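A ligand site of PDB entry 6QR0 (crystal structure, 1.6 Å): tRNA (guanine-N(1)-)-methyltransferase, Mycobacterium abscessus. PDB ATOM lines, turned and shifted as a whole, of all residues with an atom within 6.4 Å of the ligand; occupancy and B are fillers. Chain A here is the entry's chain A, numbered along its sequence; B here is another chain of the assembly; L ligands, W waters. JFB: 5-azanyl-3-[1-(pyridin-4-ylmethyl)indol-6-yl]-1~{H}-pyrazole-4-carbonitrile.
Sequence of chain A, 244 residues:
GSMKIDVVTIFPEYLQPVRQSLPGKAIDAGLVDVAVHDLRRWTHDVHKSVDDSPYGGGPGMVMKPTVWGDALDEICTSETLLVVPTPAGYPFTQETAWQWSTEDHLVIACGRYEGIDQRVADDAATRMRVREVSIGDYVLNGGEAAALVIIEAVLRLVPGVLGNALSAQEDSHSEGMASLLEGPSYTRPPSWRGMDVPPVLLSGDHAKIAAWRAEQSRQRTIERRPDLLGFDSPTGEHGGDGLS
O of Val 133 sits close to N08 of the ligand, 3.4 Å away.
Residues that only touch the ligand: Pro 85 (3.3 Å), Pro 87 (3.4 Å), Gly 111 (3.4 Å), Arg 112 (3.6 Å), Tyr 113 (3.2 Å), Glu 114 (3.5 Å), Val 139 (3.6 Å), Asn 141 (3.3 Å), Gly 142 (3.5 Å), Gly 143 (3.5 Å) and Ala 146 (3.5 Å).
Hydrophobic or aromatic side chains that line the ligand: Pro 85, Pro 87, Ile 135, Tyr 138, Val 139, Leu 140 and Ala 146.
19 residues have an atom within 4 Å of the ligand: Pro 85, Thr 86, Pro 87, Gly 111, Arg 112, Tyr 113, Glu 114, Val 133, Ser 134, Ile 135, Gly 136, Tyr 138, Val 139, Leu 140, Asn 141, Gly 142, Gly 143, Ala 146 and Glu 182 of chain B.
The nearest printed residue that does not touch the ligand is Gly 115 (4.04 Å).
The backbone NH of Ala 88 sits at hydrogen-bond distance from the side-chain hydroxyl of Thr 86 (3.0 Å).
O of Gly 136 lies within hydrogen-bond range of OG of Ser 134, 3.1 Å away.
The backbone carbonyl oxygen (O) of Gly 111 is in hydrogen-bond range of the backbone NH (N) of Gly 143, at 2.9 Å.
The side-chain carboxylate (OE1) of Glu 144 is in salt-bridge range of the guanidinium group (NE) of Arg 112 (2.8 Å).
The backbone NH (N) of Thr 86 sits at hydrogen-bond distance from the backbone carbonyl oxygen (O) of Val 133 (2.9 Å).
N of Val 133 sits at hydrogen-bond distance from O of Val 84 (3.1 Å).
The guanidinium group (NE) of Arg 156 of chain B is in hydrogen-bond range of the side-chain amide oxygen (OD1) of Asn 141, 3.0 Å away.
OH of Tyr 138 lies within hydrogen-bond range of O of Ile 135 (3.2 Å).
N of Ile 135 is in hydrogen-bond range of N08 of the ligand, at 3.5 Å.
The backbone carbonyl oxygen (O) of Tyr 138 is in hydrogen-bond range of a nitrogen (N03) of the ligand (2.6 Å).
OE1 of Glu 182 of chain B lies within hydrogen-bond range of N20 of the ligand (2.9 Å).
N of Leu 140 sits at hydrogen-bond distance from N04 of the ligand (3.0 Å).
The backbone NH of Thr 86 lies within hydrogen-bond range of a nitrogen (N08) of the ligand, 3.5 Å away.
A nitrogen (N01) of the ligand is in hydrogen-bond range of the side-chain hydroxyl of Ser 134 (3.0 Å).
O of Gly 136 sits at hydrogen-bond distance from N01 of the ligand (2.9 Å).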
ATOM      1  N   VAL A  84      -0.280  -2.820 -10.692  1.00  0.00           N
ATOM      2  CA  VAL A  84      -0.002  -2.134  -9.432  1.00  0.00           C
ATOM      3  C   VAL A  84       0.309  -0.672  -9.714  1.00  0.00           C
ATOM      4  O   VAL A  84       1.422  -0.332 -10.112  1.00  0.00           O
ATOM      5  CB  VAL A  84       1.191  -2.762  -8.679  1.00  0.00           C
ATOM      6  CG1 VAL A  84       1.350  -2.120  -7.316  1.00  0.00           C
ATOM      7  CG2 VAL A  84       1.015  -4.291  -8.561  1.00  0.00           C
ATOM      8  N   PRO A  85      -0.688   0.203  -9.530  1.00  0.00           N
ATOM      9  CA  PRO A  85      -0.392   1.629  -9.683  1.00  0.00           C
ATOM     10  C   PRO A  85       0.668   2.074  -8.690  1.00  0.00           C
ATOM     11  O   PRO A  85       0.674   1.639  -7.542  1.00  0.00           O
ATOM     12  CB  PRO A  85      -1.749   2.295  -9.389  1.00  0.00           C
ATOM     13  CG  PRO A  85      -2.764   1.260  -9.799  1.00  0.00           C
ATOM     14  CD  PRO A  85      -2.130  -0.076  -9.395  1.00  0.00           C
ATOM     15  N   THR A  86       1.586   2.936  -9.150  1.00  0.00           N
ATOM     16  CA  THR A  86       2.615   3.507  -8.282  1.00  0.00           C
ATOM     17  C   THR A  86       3.183   4.719  -8.984  1.00  0.00           C
ATOM     18  O   THR A  86       3.308   4.697 -10.193  1.00  0.00           O
ATOM     19  CB  THR A  86       3.728   2.493  -7.946  1.00  0.00           C
ATOM     20  OG1 THR A  86       4.894   3.197  -7.464  1.00  0.00           O
ATOM     21  CG2 THR A  86       4.098   1.640  -9.137  1.00  0.00           C
ATOM     22  N   PRO A  87       3.533   5.760  -8.211  1.00  0.00           N
ATOM     23  CA  PRO A  87       4.160   6.929  -8.840  1.00  0.00           C
ATOM     24  C   PRO A  87       5.519   6.566  -9.455  1.00  0.00           C
ATOM     25  O   PRO A  87       5.992   7.283 -10.338  1.00  0.00           O
ATOM     26  CB  PRO A  87       4.298   7.929  -7.690  1.00  0.00           C
ATOM     27  CG  PRO A  87       4.161   7.156  -6.453  1.00  0.00           C
ATOM     28  CD  PRO A  87       3.341   5.931  -6.762  1.00  0.00           C
ATOM     29  N   ALA A  88       6.110   5.457  -9.027  1.00  0.00           N
ATOM     30  CA  ALA A  88       7.369   5.003  -9.616  1.00  0.00           C
ATOM     31  C   ALA A  88       7.192   3.995 -10.748  1.00  0.00           C
ATOM     32  O   ALA A  88       8.138   3.286 -11.106  1.00  0.00           O
ATOM     33  CB  ALA A  88       8.272   4.403  -8.515  1.00  0.00           C
ATOM     34  N   CYS A 110      -4.557  -1.635  -5.307  1.00  0.00           N
ATOM     35  CA  CYS A 110      -4.480  -0.221  -4.982  1.00  0.00           C
ATOM     36  C   CYS A 110      -3.804   0.008  -3.650  1.00  0.00           C
ATOM     37  O   CYS A 110      -4.344  -0.357  -2.608  1.00  0.00           O
ATOM     38  CB  CYS A 110      -5.872   0.404  -4.934  1.00  0.00           C
ATOM     39  SG  CYS A 110      -6.773   0.339  -6.490  1.00  0.00           S
ATOM     40  N   GLY A 111      -2.651   0.658  -3.677  1.00  0.00           N
ATOM     41  CA  GLY A 111      -1.994   1.030  -2.435  1.00  0.00           C
ATOM     42  C   GLY A 111      -2.448   2.357  -1.835  1.00  0.00           C
ATOM     43  O   GLY A 111      -3.165   3.152  -2.462  1.00  0.00           O
ATOM     44  N   ARG A 112      -2.033   2.559  -0.594  1.00  0.00           N
ATOM     45  CA  ARG A 112      -2.176   3.838   0.096  1.00  0.00           C
ATOM     46  C   ARG A 112      -0.886   4.069   0.883  1.00  0.00           C
ATOM     47  O   ARG A 112       0.028   3.239   0.828  1.00  0.00           O
ATOM     48  CB  ARG A 112      -3.414   3.838   1.006  1.00  0.00           C
ATOM     49  CG  ARG A 112      -4.746   4.040   0.266  1.00  0.00           C
ATOM     50  CD  ARG A 112      -5.083   5.522   0.161  1.00  0.00           C
ATOM     51  NE  ARG A 112      -5.944   5.818  -0.986  1.00  0.00           N
ATOM     52  CZ  ARG A 112      -6.534   6.993  -1.172  1.00  0.00           C
ATOM     53  NH1 ARG A 112      -6.368   7.973  -0.270  1.00  0.00           N
ATOM     54  NH2 ARG A 112      -7.289   7.199  -2.243  1.00  0.00           N
ATOM     55  N   TYR A 113      -0.816   5.197   1.589  1.00  0.00           N
ATOM     56  CA  TYR A 113       0.381   5.551   2.362  1.00  0.00           C
ATOM     57  C   TYR A 113       1.584   5.653   1.425  1.00  0.00           C
ATOM     58  O   TYR A 113       1.504   6.304   0.379  1.00  0.00           O
ATOM     59  CB  TYR A 113       0.597   4.528   3.483  1.00  0.00           C
ATOM     60  CG  TYR A 113      -0.682   4.278   4.255  1.00  0.00           C
ATOM     61  CD1 TYR A 113      -1.262   5.286   5.002  1.00  0.00           C
ATOM     62  CD2 TYR A 113      -1.321   3.055   4.199  1.00  0.00           C
ATOM     63  CE1 TYR A 113      -2.436   5.073   5.689  1.00  0.00           C
ATOM     64  CE2 TYR A 113      -2.496   2.837   4.877  1.00  0.00           C
ATOM     65  CZ  TYR A 113      -3.053   3.851   5.630  1.00  0.00           C
ATOM     66  OH  TYR A 113      -4.228   3.639   6.317  1.00  0.00           O
ATOM     67  N   GLU A 114       2.704   5.032   1.762  1.00  0.00           N
ATOM     68  CA  GLU A 114       3.856   5.137   0.872  1.00  0.00           C
ATOM     69  C   GLU A 114       3.841   4.087  -0.228  1.00  0.00           C
ATOM     70  O   GLU A 114       4.658   4.133  -1.151  1.00  0.00           O
ATOM     71  CB  GLU A 114       5.166   5.056   1.666  1.00  0.00           C
ATOM     72  CG  GLU A 114       5.405   6.304   2.502  1.00  0.00           C
ATOM     73  CD  GLU A 114       5.299   7.573   1.660  1.00  0.00           C
ATOM     74  OE1 GLU A 114       6.149   7.757   0.756  1.00  0.00           O
ATOM     75  OE2 GLU A 114       4.370   8.366   1.905  1.00  0.00           O
ATOM     76  N   GLY A 115       2.889   3.144  -0.154  1.00  0.00           N
ATOM     77  CA  GLY A 115       2.800   2.074  -1.120  1.00  0.00           C
ATOM     78  C   GLY A 115       2.838   0.714  -0.431  1.00  0.00           C
ATOM     79  O   GLY A 115       2.684   0.628   0.788  1.00  0.00           O
ATOM     80  N   ILE A 116       3.033  -0.322  -1.240  1.00  0.00           N
ATOM     81  CA  ILE A 116       2.992  -1.726  -0.792  1.00  0.00           C
ATOM     82  C   ILE A 116       4.401  -2.267  -0.658  1.00  0.00           C
ATOM     83  O   ILE A 116       5.246  -2.000  -1.496  1.00  0.00           O
ATOM     84  CB  ILE A 116       2.193  -2.593  -1.776  1.00  0.00           C
ATOM     85  CG1 ILE A 116       0.800  -1.984  -1.990  1.00  0.00           C
ATOM     86  CG2 ILE A 116       2.086  -4.036  -1.278  1.00  0.00           C
ATOM     87  CD1 ILE A 116      -0.013  -2.657  -3.060  1.00  0.00           C
ATOM     88  N   VAL A 133       2.742   0.476 -12.834  1.00  0.00           N
ATOM     89  CA  VAL A 133       2.526   1.550 -13.798  1.00  0.00           C
ATOM     90  C   VAL A 133       2.108   2.838 -13.115  1.00  0.00           C
ATOM     91  O   VAL A 133       1.527   2.809 -12.035  1.00  0.00           O
ATOM     92  CB  VAL A 133       1.425   1.207 -14.841  1.00  0.00           C
ATOM     93  CG1 VAL A 133       1.829   0.006 -15.696  1.00  0.00           C
ATOM     94  CG2 VAL A 133       0.063   0.946 -14.165  1.00  0.00           C
ATOM     95  N   SER A 134       2.373   3.966 -13.789  1.00  0.00           N
ATOM     96  CA  SER A 134       1.932   5.287 -13.327  1.00  0.00           C
ATOM     97  C   SER A 134       1.065   5.956 -14.377  1.00  0.00           C
ATOM     98  O   SER A 134       1.404   5.910 -15.568  1.00  0.00           O
ATOM     99  CB  SER A 134       3.141   6.188 -13.065  1.00  0.00           C
ATOM    100  OG  SER A 134       2.726   7.529 -12.830  1.00  0.00           O
ATOM    101  N   ILE A 135      -0.027   6.616 -13.960  1.00  0.00           N
ATOM    102  CA  ILE A 135      -0.905   7.261 -14.936  1.00  0.00           C
ATOM    103  C   ILE A 135      -0.481   8.701 -15.291  1.00  0.00           C
ATOM    104  O   ILE A 135      -1.085   9.321 -16.168  1.00  0.00           O
ATOM    105  CB  ILE A 135      -2.384   7.264 -14.469  1.00  0.00           C
ATOM    106  CG1 ILE A 135      -2.571   8.010 -13.134  1.00  0.00           C
ATOM    107  CG2 ILE A 135      -2.920   5.807 -14.418  1.00  0.00           C
ATOM    108  CD1 ILE A 135      -4.016   8.529 -12.934  1.00  0.00           C
ATOM    109  N   GLY A 136       0.560   9.225 -14.644  1.00  0.00           N
ATOM    110  CA  GLY A 136       1.043  10.546 -15.021  1.00  0.00           C
ATOM    111  C   GLY A 136       2.004  11.147 -14.017  1.00  0.00           C
ATOM    112  O   GLY A 136       2.223  10.600 -12.947  1.00  0.00           O
ATOM    113  N   ASP A 137       2.585  12.297 -14.372  1.00  0.00           N
ATOM    114  CA  ASP A 137       3.633  12.866 -13.552  1.00  0.00           C
ATOM    115  C   ASP A 137       3.115  13.864 -12.518  1.00  0.00           C
ATOM    116  O   ASP A 137       3.392  15.066 -12.576  1.00  0.00           O
ATOM    117  CB  ASP A 137       4.688  13.525 -14.444  1.00  0.00           C
ATOM    118  CG  ASP A 137       5.467  12.503 -15.249  1.00  0.00           C
ATOM    119  OD1 ASP A 137       5.528  11.339 -14.790  1.00  0.00           O
ATOM    120  OD2 ASP A 137       6.003  12.845 -16.312  1.00  0.00           O
ATOM    121  N   TYR A 138       2.368  13.318 -11.567  1.00  0.00           N
ATOM    122  CA  TYR A 138       1.812  14.038 -10.438  1.00  0.00           C
ATOM    123  C   TYR A 138       1.662  12.991  -9.359  1.00  0.00           C
ATOM    124  O   TYR A 138       1.715  11.786  -9.643  1.00  0.00           O
ATOM    125  CB  TYR A 138       0.456  14.691 -10.775  1.00  0.00           C
ATOM    126  CG  TYR A 138      -0.365  13.827 -11.690  1.00  0.00           C
ATOM    127  CD1 TYR A 138      -1.036  12.696 -11.213  1.00  0.00           C
ATOM    128  CD2 TYR A 138      -0.450  14.112 -13.049  1.00  0.00           C
ATOM    129  CE1 TYR A 138      -1.747  11.875 -12.064  1.00  0.00           C
ATOM    130  CE2 TYR A 138      -1.181  13.316 -13.915  1.00  0.00           C
ATOM    131  CZ  TYR A 138      -1.834  12.189 -13.417  1.00  0.00           C
ATOM    132  OH  TYR A 138      -2.547  11.386 -14.280  1.00  0.00           O
ATOM    133  N   VAL A 139       1.462  13.456  -8.132  1.00  0.00           N
ATOM    134  CA  VAL A 139       1.397  12.564  -6.988  1.00  0.00           C
ATOM    135  C   VAL A 139      -0.031  12.503  -6.447  1.00  0.00           C
ATOM    136  O   VAL A 139      -0.658  13.539  -6.224  1.00  0.00           O
ATOM    137  CB  VAL A 139       2.331  13.017  -5.878  1.00  0.00           C
ATOM    138  CG1 VAL A 139       2.341  11.998  -4.739  1.00  0.00           C
ATOM    139  CG2 VAL A 139       3.730  13.230  -6.442  1.00  0.00           C
ATOM    140  N   LEU A 140      -0.540  11.286  -6.264  1.00  0.00           N
ATOM    141  CA  LEU A 140      -1.856  11.049  -5.675  1.00  0.00           C
ATOM    142  C   LEU A 140      -1.698  10.543  -4.251  1.00  0.00           C
ATOM    143  O   LEU A 140      -0.580  10.319  -3.797  1.00  0.00           O
ATOM    144  CB  LEU A 140      -2.638  10.031  -6.506  1.00  0.00           C
ATOM    145  CG  LEU A 140      -2.792  10.392  -7.993  1.00  0.00           C
ATOM    146  CD1 LEU A 140      -3.361   9.238  -8.782  1.00  0.00           C
ATOM    147  CD2 LEU A 140      -3.692  11.626  -8.133  1.00  0.00           C
ATOM    148  N   ASN A 141      -2.819  10.335  -3.558  1.00  0.00           N
ATOM    149  CA  ASN A 141      -2.797   9.767  -2.208  1.00  0.00           C
ATOM    150  C   ASN A 141      -2.764   8.242  -2.230  1.00  0.00           C
ATOM    151  O   ASN A 141      -2.444   7.593  -1.206  1.00  0.00           O
ATOM    152  CB  ASN A 141      -4.019  10.219  -1.417  1.00  0.00           C
ATOM    153  CG  ASN A 141      -3.915  11.658  -0.956  1.00  0.00           C
ATOM    154  OD1 ASN A 141      -2.822  12.134  -0.623  1.00  0.00           O
ATOM    155  ND2 ASN A 141      -5.039  12.356  -0.939  1.00  0.00           N
ATOM    156  N   GLY A 142      -3.106   7.650  -3.370  1.00  0.00           N
ATOM    157  CA  GLY A 142      -3.207   6.208  -3.439  1.00  0.00           C
ATOM    158  C   GLY A 142      -3.595   5.761  -4.822  1.00  0.00           C
ATOM    159  O   GLY A 142      -3.760   6.578  -5.732  1.00  0.00           O
ATOM    160  N   GLY A 143      -3.730   4.447  -4.994  1.00  0.00           N
ATOM    161  CA  GLY A 143      -3.959   3.900  -6.320  1.00  0.00           C
ATOM    162  C   GLY A 143      -5.370   3.935  -6.880  1.00  0.00           C
ATOM    163  O   GLY A 143      -5.561   3.616  -8.044  1.00  0.00           O
ATOM    164  N   GLU A 144      -6.348   4.324  -6.072  1.00  0.00           N
ATOM    165  CA  GLU A 144      -7.748   4.214  -6.494  1.00  0.00           C
ATOM    166  C   GLU A 144      -8.096   5.093  -7.696  1.00  0.00           C
ATOM    167  O   GLU A 144      -8.755   4.627  -8.631  1.00  0.00           O
ATOM    168  CB  GLU A 144      -8.678   4.551  -5.335  1.00  0.00           C
ATOM    169  CG  GLU A 144      -8.694   3.461  -4.246  1.00  0.00           C
ATOM    170  CD  GLU A 144      -7.540   3.523  -3.264  1.00  0.00           C
ATOM    171  OE1 GLU A 144      -6.730   4.477  -3.304  1.00  0.00           O
ATOM    172  OE2 GLU A 144      -7.434   2.582  -2.451  1.00  0.00           O
ATOM    173  N   ALA A 146      -6.086   6.112  -9.915  1.00  0.00           N
ATOM    174  CA  ALA A 146      -5.367   5.525 -11.038  1.00  0.00           C
ATOM    175  C   ALA A 146      -6.120   4.314 -11.572  1.00  0.00           C
ATOM    176  O   ALA A 146      -6.218   4.115 -12.779  1.00  0.00           O
ATOM    177  CB  ALA A 146      -3.933   5.140 -10.625  1.00  0.00           C
ATOM    178  N   ILE A 150      -7.339   3.707 -15.377  1.00  0.00           N
ATOM    179  CA  ILE A 150      -6.963   2.516 -16.119  1.00  0.00           C
ATOM    180  C   ILE A 150      -8.161   1.701 -16.577  1.00  0.00           C
ATOM    181  O   ILE A 150      -8.226   1.251 -17.734  1.00  0.00           O
ATOM    182  CB  ILE A 150      -6.023   1.643 -15.273  1.00  0.00           C
ATOM    183  CG1 ILE A 150      -4.693   2.373 -15.050  1.00  0.00           C
ATOM    184  CG2 ILE A 150      -5.822   0.270 -15.929  1.00  0.00           C
ATOM    185  CD1 ILE A 150      -3.827   1.807 -13.922  1.00  0.00           C
ATOM    186  N   ARG B 156      -4.134  17.626  -1.904  1.00  0.00           N
ATOM    187  CA  ARG B 156      -3.124  17.166  -0.943  1.00  0.00           C
ATOM    188  C   ARG B 156      -1.987  18.191  -0.756  1.00  0.00           C
ATOM    189  O   ARG B 156      -1.168  18.054   0.151  1.00  0.00           O
ATOM    190  CB  ARG B 156      -2.574  15.809  -1.362  1.00  0.00           C
ATOM    191  CG  ARG B 156      -1.864  15.777  -2.681  1.00  0.00           C
ATOM    192  CD  ARG B 156      -1.623  14.331  -3.104  1.00  0.00           C
ATOM    193  NE  ARG B 156      -0.728  13.602  -2.206  1.00  0.00           N
ATOM    194  CZ  ARG B 156       0.591  13.779  -2.154  1.00  0.00           C
ATOM    195  NH1 ARG B 156       1.186  14.690  -2.927  1.00  0.00           N
ATOM    196  NH2 ARG B 156       1.315  13.050  -1.320  1.00  0.00           N
ATOM    197  N   GLU B 182      10.739   7.182  -6.858  1.00  0.00           N
ATOM    198  CA  GLU B 182      10.951   6.624  -5.534  1.00  0.00           C
ATOM    199  C   GLU B 182      11.369   5.167  -5.649  1.00  0.00           C
ATOM    200  O   GLU B 182      10.930   4.453  -6.554  1.00  0.00           O
ATOM    201  CB  GLU B 182       9.678   6.741  -4.684  1.00  0.00           C
ATOM    202  CG  GLU B 182       9.453   8.132  -4.098  1.00  0.00           C
ATOM    203  CD  GLU B 182       8.003   8.357  -3.723  1.00  0.00           C
ATOM    204  OE1 GLU B 182       7.742   8.869  -2.605  1.00  0.00           O
ATOM    205  OE2 GLU B 182       7.125   8.032  -4.538  1.00  0.00           O
HETATM  206  C10 JFB L   1      -0.287   5.269  -7.025  1.00  0.00           C
HETATM  207  C13 JFB L   1       0.177   6.178  -4.399  1.00  0.00           C
HETATM  208  C17 JFB L   1       2.162   7.974  -2.494  1.00  0.00           C
HETATM  209  C21 JFB L   1       3.948   9.571  -2.480  1.00  0.00           C
HETATM  210  C22 JFB L   1       2.604   9.299  -2.400  1.00  0.00           C
HETATM  211  C24 JFB L   1      -0.068   4.213  -3.306  1.00  0.00           C
HETATM  212  N01 JFB L   1       0.577   8.936 -11.247  1.00  0.00           N
HETATM  213  C02 JFB L   1       0.478   8.641  -9.839  1.00  0.00           C
HETATM  214  N03 JFB L   1       0.690   9.497  -8.837  1.00  0.00           N
HETATM  215  N04 JFB L   1       0.504   8.811  -7.641  1.00  0.00           N
HETATM  216  C05 JFB L   1       0.142   7.606  -7.886  1.00  0.00           C
HETATM  217  C06 JFB L   1       0.155   7.409  -9.287  1.00  0.00           C
HETATM  218  C07 JFB L   1      -0.161   6.200 -10.098  1.00  0.00           C
HETATM  219  N08 JFB L   1      -0.395   5.341 -10.743  1.00  0.00           N
HETATM  220  C09 JFB L   1      -0.034   6.601  -6.761  1.00  0.00           C
HETATM  221  C11 JFB L   1      -0.339   4.371  -5.961  1.00  0.00           C
HETATM  222  C12 JFB L   1      -0.114   4.849  -4.627  1.00  0.00           C
HETATM  223  C14 JFB L   1       0.239   7.073  -5.461  1.00  0.00           C
HETATM  224  N15 JFB L   1       0.363   6.367  -3.046  1.00  0.00           N
HETATM  225  C16 JFB L   1       0.675   7.635  -2.403  1.00  0.00           C
HETATM  226  C18 JFB L   1       3.171   6.934  -2.646  1.00  0.00           C
HETATM  227  C19 JFB L   1       4.523   7.299  -2.714  1.00  0.00           C
HETATM  228  N20 JFB L   1       4.866   8.551  -2.628  1.00  0.00           N
HETATM  229  C23 JFB L   1       0.208   5.178  -2.387  1.00  0.00           C
HETATM  230  O   HOH W   1       1.888   1.671  -4.687  1.00  0.00           O
